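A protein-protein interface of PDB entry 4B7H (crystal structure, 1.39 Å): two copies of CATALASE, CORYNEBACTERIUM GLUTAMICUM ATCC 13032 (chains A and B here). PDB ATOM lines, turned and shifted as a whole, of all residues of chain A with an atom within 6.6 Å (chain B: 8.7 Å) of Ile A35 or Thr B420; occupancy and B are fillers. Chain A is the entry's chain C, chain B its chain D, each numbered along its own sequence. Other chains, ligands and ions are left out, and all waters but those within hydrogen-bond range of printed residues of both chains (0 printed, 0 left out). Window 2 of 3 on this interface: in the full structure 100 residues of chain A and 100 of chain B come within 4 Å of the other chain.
The backbone carbonyl oxygen (O) of Pro A31 lies within hydrogen-bond range of the backbone NH (N) of Leu B409 (2.9 Å). The side-chain carboxylate (OD1) of Asp B410 lies within hydrogen-bond range of the side-chain hydroxyl (OG) of Ser A32 (2.7 Å). The backbone NH of Glu A33 is in hydrogen-bond range of the side-chain carboxylate of Asp B410. ND2 of Asn A34 lies within hydrogen-bond range of OD1 of Asp B410 (3.5 Å). The backbone carbonyl oxygen (O) of Asp B414 lies within hydrogen-bond range of the side-chain amide nitrogen (ND2) of Asn A34, 3.0 Å away. OG of Ser B416 is in hydrogen-bond range of ND2 of Asn A34 (2.9 Å).
OG of Ser A32 sits at hydrogen-bond distance from N of Asn A34, at 2.9 Å. The backbone NH (N) of Ala A37 is in hydrogen-bond range of the side-chain carboxylate (OD2) of Asp A49, at 2.9 Å. OD2 of Asp B410 sits at hydrogen-bond distance from N of Gly B407. The side-chain hydroxyl (OH) of Tyr B422 sits close to the backbone carbonyl oxygen (O) of Leu B409, 3.4 Å away. The side-chain amide oxygen (OD1) of Asn B411 is in hydrogen-bond range of the backbone NH (N) of Asp B414, 2.9 Å away. The backbone NH (N) of Ser B416 lies within hydrogen-bond range of the side-chain carboxylate (OD1) of Asp B414, at 3.0 Å.
Gly B407 touches Pro A31. CE2 of Tyr B422 touches OG of Ser A32 (3.5 Å). Gly B407 touches Glu A33 (N to CG, 3.7 Å). O of Ser B415 touches CB of Asn A34, at 3.3 Å. Thr B420 touches Ile A35. Tyr B422 touches Ile A35. Ala A37 touches Ile B428.
Ile A35 touches just these residues of chain B: Thr B420 (3.6 Å) and Tyr B422 (3.95 Å). Of the printed residues of chain B, Ala A37 touches Ile B428 (3.7 Å). Of the printed residues of chain A, Leu B409 touches Pro A31 (2.9 Å). Asn B411 touches none of the printed residues of chain A. The nearest printed residue of chain A that does not touch Thr B420 is Asn A34 (7.4 Å).
Of the 8 printed residues of chain A, 6 touch a printed residue of chain B. Printed residues of chain A that touch a printed residue of chain B: Pro A31, Ser A32, Glu A33, Asn A34, Ile A35 and Ala A37. Hydrophobic or aromatic side chains of chain A that line the printed part of chain B: Pro A31, Ile A35 and Ala A37. Along chain A the printed residues that touch a printed residue of chain B span positions 31 to 37. Among the printed residues, no Asp or Glu carboxylate lies within 4 Å of a Lys or Arg side-chain nitrogen of the other chain.
No position is printed for both chains.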
ATOM      1  N   PRO A  31       7.438   7.613 -18.781  1.00  0.00           N
ATOM      2  CA  PRO A  31       7.471   8.089 -20.167  1.00  0.00           C
ATOM      3  C   PRO A  31       6.279   8.983 -20.511  1.00  0.00           C
ATOM      4  O   PRO A  31       6.498  10.093 -21.000  1.00  0.00           O
ATOM      5  CB  PRO A  31       7.447   6.788 -20.986  1.00  0.00           C
ATOM      6  CG  PRO A  31       7.992   5.737 -20.034  1.00  0.00           C
ATOM      7  CD  PRO A  31       7.441   6.143 -18.697  1.00  0.00           C
ATOM      8  N   SER A  32       5.051   8.538 -20.240  1.00  0.00           N
ATOM      9  CA  SER A  32       3.875   9.340 -20.583  1.00  0.00           C
ATOM     10  C   SER A  32       2.751   9.205 -19.572  1.00  0.00           C
ATOM     11  O   SER A  32       2.469   8.112 -19.074  1.00  0.00           O
ATOM     12  CB  SER A  32       3.335   8.964 -21.966  1.00  0.00           C
ATOM     13  OG  SER A  32       2.283   9.844 -22.353  1.00  0.00           O
ATOM     14  N   GLU A  33       2.108  10.330 -19.280  1.00  0.00           N
ATOM     15  CA  GLU A  33       0.862  10.336 -18.522  1.00  0.00           C
ATOM     16  C   GLU A  33      -0.347  10.382 -19.450  1.00  0.00           C
ATOM     17  O   GLU A  33      -1.489  10.449 -18.981  1.00  0.00           O
ATOM     18  CB  GLU A  33       0.801  11.554 -17.597  1.00  0.00           C
ATOM     19  CG  GLU A  33       1.887  11.614 -16.533  1.00  0.00           C
ATOM     20  CD  GLU A  33       1.757  10.533 -15.459  1.00  0.00           C
ATOM     21  OE1 GLU A  33       0.834   9.680 -15.505  1.00  0.00           O
ATOM     22  OE2 GLU A  33       2.596  10.536 -14.542  1.00  0.00           O
ATOM     23  N   ASN A  34      -0.099  10.343 -20.758  1.00  0.00           N
ATOM     24  CA  ASN A  34      -1.146  10.603 -21.745  1.00  0.00           C
ATOM     25  C   ASN A  34      -1.480   9.431 -22.672  1.00  0.00           C
ATOM     26  O   ASN A  34      -2.637   9.260 -23.064  1.00  0.00           O
ATOM     27  CB  ASN A  34      -0.764  11.805 -22.612  1.00  0.00           C
ATOM     28  CG  ASN A  34      -0.696  13.100 -21.833  1.00  0.00           C
ATOM     29  OD1 ASN A  34      -1.337  13.262 -20.793  1.00  0.00           O
ATOM     30  ND2 ASN A  34       0.069  14.050 -22.354  1.00  0.00           N
ATOM     31  N   ILE A  35      -0.471   8.648 -23.052  1.00  0.00           N
ATOM     32  CA  ILE A  35      -0.648   7.593 -24.052  1.00  0.00           C
ATOM     33  C   ILE A  35      -0.137   6.260 -23.509  1.00  0.00           C
ATOM     34  O   ILE A  35       0.977   6.204 -22.989  1.00  0.00           O
ATOM     35  CB  ILE A  35       0.120   7.928 -25.360  1.00  0.00           C
ATOM     36  CG1 ILE A  35      -0.315   9.296 -25.901  1.00  0.00           C
ATOM     37  CG2 ILE A  35      -0.062   6.825 -26.415  1.00  0.00           C
ATOM     38  CD1 ILE A  35       0.400   9.720 -27.195  1.00  0.00           C
ATOM     39  N   SER A  36      -0.935   5.194 -23.644  1.00  0.00           N
ATOM     40  CA  SER A  36      -0.519   3.859 -23.208  1.00  0.00           C
ATOM     41  C   SER A  36       0.127   3.086 -24.360  1.00  0.00           C
ATOM     42  O   SER A  36      -0.076   3.415 -25.532  1.00  0.00           O
ATOM     43  CB  SER A  36      -1.691   3.072 -22.608  1.00  0.00           C
ATOM     44  OG  SER A  36      -2.802   3.010 -23.490  1.00  0.00           O
ATOM     45  N   ALA A  37       0.904   2.060 -24.022  1.00  0.00           N
ATOM     46  CA  ALA A  37       1.702   1.335 -25.010  1.00  0.00           C
ATOM     47  C   ALA A  37       0.910   0.208 -25.675  1.00  0.00           C
ATOM     48  O   ALA A  37       0.222  -0.572 -25.004  1.00  0.00           O
ATOM     49  CB  ALA A  37       2.975   0.794 -24.364  1.00  0.00           C
ATOM     50  N   ASP A  49       2.779  -2.313 -19.888  1.00  0.00           N
ATOM     51  CA  ASP A  49       2.866  -0.879 -19.655  1.00  0.00           C
ATOM     52  C   ASP A  49       2.797  -0.748 -18.137  1.00  0.00           C
ATOM     53  O   ASP A  49       1.711  -0.718 -17.536  1.00  0.00           O
ATOM     54  CB  ASP A  49       1.736  -0.122 -20.352  1.00  0.00           C
ATOM     55  CG  ASP A  49       1.923   1.377 -20.280  1.00  0.00           C
ATOM     56  OD1 ASP A  49       2.472   1.854 -19.264  1.00  0.00           O
ATOM     57  OD2 ASP A  49       1.537   2.088 -21.237  1.00  0.00           O
ATOM     58  N   GLY B 407       4.934  13.090 -18.058  1.00  0.00           N
ATOM     59  CA  GLY B 407       5.961  12.156 -18.486  1.00  0.00           C
ATOM     60  C   GLY B 407       7.046  12.835 -19.300  1.00  0.00           C
ATOM     61  O   GLY B 407       6.827  13.931 -19.838  1.00  0.00           O
ATOM     62  N   LEU B 409       8.140  12.152 -22.146  1.00  0.00           N
ATOM     63  CA  LEU B 409       7.750  12.244 -23.554  1.00  0.00           C
ATOM     64  C   LEU B 409       6.701  13.330 -23.772  1.00  0.00           C
ATOM     65  O   LEU B 409       6.503  13.792 -24.898  1.00  0.00           O
ATOM     66  CB  LEU B 409       7.187  10.903 -24.039  1.00  0.00           C
ATOM     67  CG  LEU B 409       8.146   9.709 -24.015  1.00  0.00           C
ATOM     68  CD1 LEU B 409       7.420   8.433 -24.429  1.00  0.00           C
ATOM     69  CD2 LEU B 409       9.330   9.979 -24.932  1.00  0.00           C
ATOM     70  N   ASP B 410       6.001  13.707 -22.704  1.00  0.00           N
ATOM     71  CA  ASP B 410       4.888  14.652 -22.798  1.00  0.00           C
ATOM     72  C   ASP B 410       5.419  16.087 -22.762  1.00  0.00           C
ATOM     73  O   ASP B 410       6.578  16.309 -22.414  1.00  0.00           O
ATOM     74  CB  ASP B 410       3.920  14.466 -21.620  1.00  0.00           C
ATOM     75  CG  ASP B 410       3.387  13.051 -21.478  1.00  0.00           C
ATOM     76  OD1 ASP B 410       3.124  12.369 -22.491  1.00  0.00           O
ATOM     77  OD2 ASP B 410       3.203  12.623 -20.321  1.00  0.00           O
ATOM     78  N   ASN B 411       4.569  17.061 -23.081  1.00  0.00           N
ATOM     79  CA  ASN B 411       4.994  18.465 -23.057  1.00  0.00           C
ATOM     80  C   ASN B 411       4.702  19.191 -21.739  1.00  0.00           C
ATOM     81  O   ASN B 411       5.133  20.328 -21.541  1.00  0.00           O
ATOM     82  CB  ASN B 411       4.445  19.244 -24.266  1.00  0.00           C
ATOM     83  CG  ASN B 411       2.930  19.336 -24.277  1.00  0.00           C
ATOM     84  OD1 ASN B 411       2.265  19.074 -23.273  1.00  0.00           O
ATOM     85  ND2 ASN B 411       2.376  19.714 -25.424  1.00  0.00           N
ATOM     86  N   ASP B 414      -0.404  19.692 -22.195  1.00  0.00           N
ATOM     87  CA  ASP B 414      -1.632  19.125 -22.749  1.00  0.00           C
ATOM     88  C   ASP B 414      -1.622  17.599 -22.777  1.00  0.00           C
ATOM     89  O   ASP B 414      -0.659  16.964 -22.341  1.00  0.00           O
ATOM     90  CB  ASP B 414      -1.949  19.719 -24.133  1.00  0.00           C
ATOM     91  CG  ASP B 414      -0.896  19.376 -25.185  1.00  0.00           C
ATOM     92  OD1 ASP B 414      -0.383  18.237 -25.201  1.00  0.00           O
ATOM     93  OD2 ASP B 414      -0.587  20.247 -26.020  1.00  0.00           O
ATOM     94  N   SER B 415      -2.692  17.036 -23.327  1.00  0.00           N
ATOM     95  CA  SER B 415      -2.942  15.600 -23.310  1.00  0.00           C
ATOM     96  C   SER B 415      -2.319  14.818 -24.467  1.00  0.00           C
ATOM     97  O   SER B 415      -2.605  13.630 -24.612  1.00  0.00           O
ATOM     98  CB  SER B 415      -4.449  15.366 -23.352  1.00  0.00           C
ATOM     99  OG  SER B 415      -4.970  15.910 -24.551  1.00  0.00           O
ATOM    100  N   SER B 416      -1.486  15.464 -25.287  1.00  0.00           N
ATOM    101  CA  SER B 416      -0.876  14.806 -26.455  1.00  0.00           C
ATOM    102  C   SER B 416      -1.924  14.338 -27.470  1.00  0.00           C
ATOM    103  O   SER B 416      -1.816  13.241 -28.031  1.00  0.00           O
ATOM    104  CB  SER B 416       0.023  13.623 -26.051  1.00  0.00           C
ATOM    105  OG  SER B 416       1.035  14.011 -25.139  1.00  0.00           O
ATOM    106  N   SER B 417      -2.956  15.154 -27.684  1.00  0.00           N
ATOM    107  CA  SER B 417      -3.926  14.874 -28.739  1.00  0.00           C
ATOM    108  C   SER B 417      -3.351  15.410 -30.066  1.00  0.00           C
ATOM    109  O   SER B 417      -2.127  15.539 -30.197  1.00  0.00           O
ATOM    110  CB  SER B 417      -5.287  15.485 -28.385  1.00  0.00           C
ATOM    111  OG  SER B 417      -6.280  15.109 -29.318  1.00  0.00           O
ATOM    112  N   ASN B 418      -4.205  15.713 -31.044  1.00  0.00           N
ATOM    113  CA  ASN B 418      -3.739  16.184 -32.352  1.00  0.00           C
ATOM    114  C   ASN B 418      -2.804  15.165 -33.004  1.00  0.00           C
ATOM    115  O   ASN B 418      -1.843  15.524 -33.681  1.00  0.00           O
ATOM    116  CB  ASN B 418      -3.038  17.544 -32.233  1.00  0.00           C
ATOM    117  CG  ASN B 418      -3.835  18.536 -31.417  1.00  0.00           C
ATOM    118  OD1 ASN B 418      -4.987  18.807 -31.720  1.00  0.00           O
ATOM    119  ND2 ASN B 418      -3.228  19.069 -30.364  1.00  0.00           N
ATOM    120  N   HIS B 419      -3.038  14.123 -32.858  1.00  0.00           N
ATOM    121  CA  HIS B 419      -2.351  12.917 -33.316  1.00  0.00           C
ATOM    122  C   HIS B 419      -0.853  12.924 -33.055  1.00  0.00           C
ATOM    123  O   HIS B 419      -0.047  12.610 -33.929  1.00  0.00           O
ATOM    124  CB  HIS B 419      -2.717  12.600 -34.771  1.00  0.00           C
ATOM    125  CG  HIS B 419      -4.157  12.232 -34.929  1.00  0.00           C
ATOM    126  ND1 HIS B 419      -5.159  13.173 -35.043  1.00  0.00           N
ATOM    127  CD2 HIS B 419      -4.752  11.028 -35.093  1.00  0.00           C
ATOM    128  CE1 HIS B 419      -6.314  12.559 -35.227  1.00  0.00           C
ATOM    129  NE2 HIS B 419      -6.094  11.257 -35.259  1.00  0.00           N
ATOM    130  N   THR B 420      -0.510  13.081 -31.839  1.00  0.00           N
ATOM    131  CA  THR B 420       0.858  12.998 -31.351  1.00  0.00           C
ATOM    132  C   THR B 420       1.268  11.535 -31.212  1.00  0.00           C
ATOM    133  O   THR B 420       0.519  10.725 -30.653  1.00  0.00           O
ATOM    134  CB  THR B 420       0.966  13.671 -29.968  1.00  0.00           C
ATOM    135  OG1 THR B 420       0.603  15.053 -30.080  1.00  0.00           O
ATOM    136  CG2 THR B 420       2.378  13.561 -29.410  1.00  0.00           C
ATOM    137  N   SER B 421       2.444  11.203 -31.742  1.00  0.00           N
ATOM    138  CA  SER B 421       3.052   9.888 -31.549  1.00  0.00           C
ATOM    139  C   SER B 421       4.455  10.005 -30.955  1.00  0.00           C
ATOM    140  O   SER B 421       5.186  10.961 -31.247  1.00  0.00           O
ATOM    141  CB  SER B 421       3.129   9.135 -32.879  1.00  0.00           C
ATOM    142  OG  SER B 421       1.838   8.811 -33.366  1.00  0.00           O
ATOM    143  N   TYR B 422       4.842   9.017 -30.151  1.00  0.00           N
ATOM    144  CA  TYR B 422       6.157   9.011 -29.522  1.00  0.00           C
ATOM    145  C   TYR B 422       7.083   7.933 -30.082  1.00  0.00           C
ATOM    146  O   TYR B 422       8.291   7.962 -29.837  1.00  0.00           O
ATOM    147  CB  TYR B 422       6.025   8.779 -28.023  1.00  0.00           C
ATOM    148  CG  TYR B 422       5.285   9.852 -27.245  1.00  0.00           C
ATOM    149  CD1 TYR B 422       5.359  11.196 -27.606  1.00  0.00           C
ATOM    150  CD2 TYR B 422       4.511   9.513 -26.141  1.00  0.00           C
ATOM    151  CE1 TYR B 422       4.695  12.173 -26.869  1.00  0.00           C
ATOM    152  CE2 TYR B 422       3.845  10.476 -25.406  1.00  0.00           C
ATOM    153  CZ  TYR B 422       3.939  11.801 -25.776  1.00  0.00           C
ATOM    154  OH  TYR B 422       3.282  12.759 -25.043  1.00  0.00           O
ATOM    155  N   GLY B 423       6.521   6.966 -30.799  1.00  0.00           N
ATOM    156  CA  GLY B 423       7.320   5.903 -31.380  1.00  0.00           C
ATOM    157  C   GLY B 423       7.629   4.737 -30.451  1.00  0.00           C
ATOM    158  O   GLY B 423       6.902   4.476 -29.485  1.00  0.00           O
ATOM    159  N   ALA B 425       8.571   2.014 -27.866  1.00  0.00           N
ATOM    160  CA  ALA B 425       8.614   2.019 -26.406  1.00  0.00           C
ATOM    161  C   ALA B 425       9.847   1.274 -25.904  1.00  0.00           C
ATOM    162  O   ALA B 425       9.735   0.225 -25.273  1.00  0.00           O
ATOM    163  CB  ALA B 425       7.328   1.408 -25.839  1.00  0.00           C
ATOM    164  N   ILE B 428      10.328  -0.152 -22.381  1.00  0.00           N
ATOM    165  CA  ILE B 428       9.773  -1.468 -22.096  1.00  0.00           C
ATOM    166  C   ILE B 428      10.765  -2.503 -22.639  1.00  0.00           C
ATOM    167  O   ILE B 428      11.389  -3.230 -21.864  1.00  0.00           O
ATOM    168  CB  ILE B 428       8.357  -1.638 -22.687  1.00  0.00           C
ATOM    169  CG1 ILE B 428       7.468  -0.476 -22.239  1.00  0.00           C
ATOM    170  CG2 ILE B 428       7.759  -2.985 -22.266  1.00  0.00           C
ATOM    171  CD1 ILE B 428       6.040  -0.555 -22.749  1.00  0.00           C
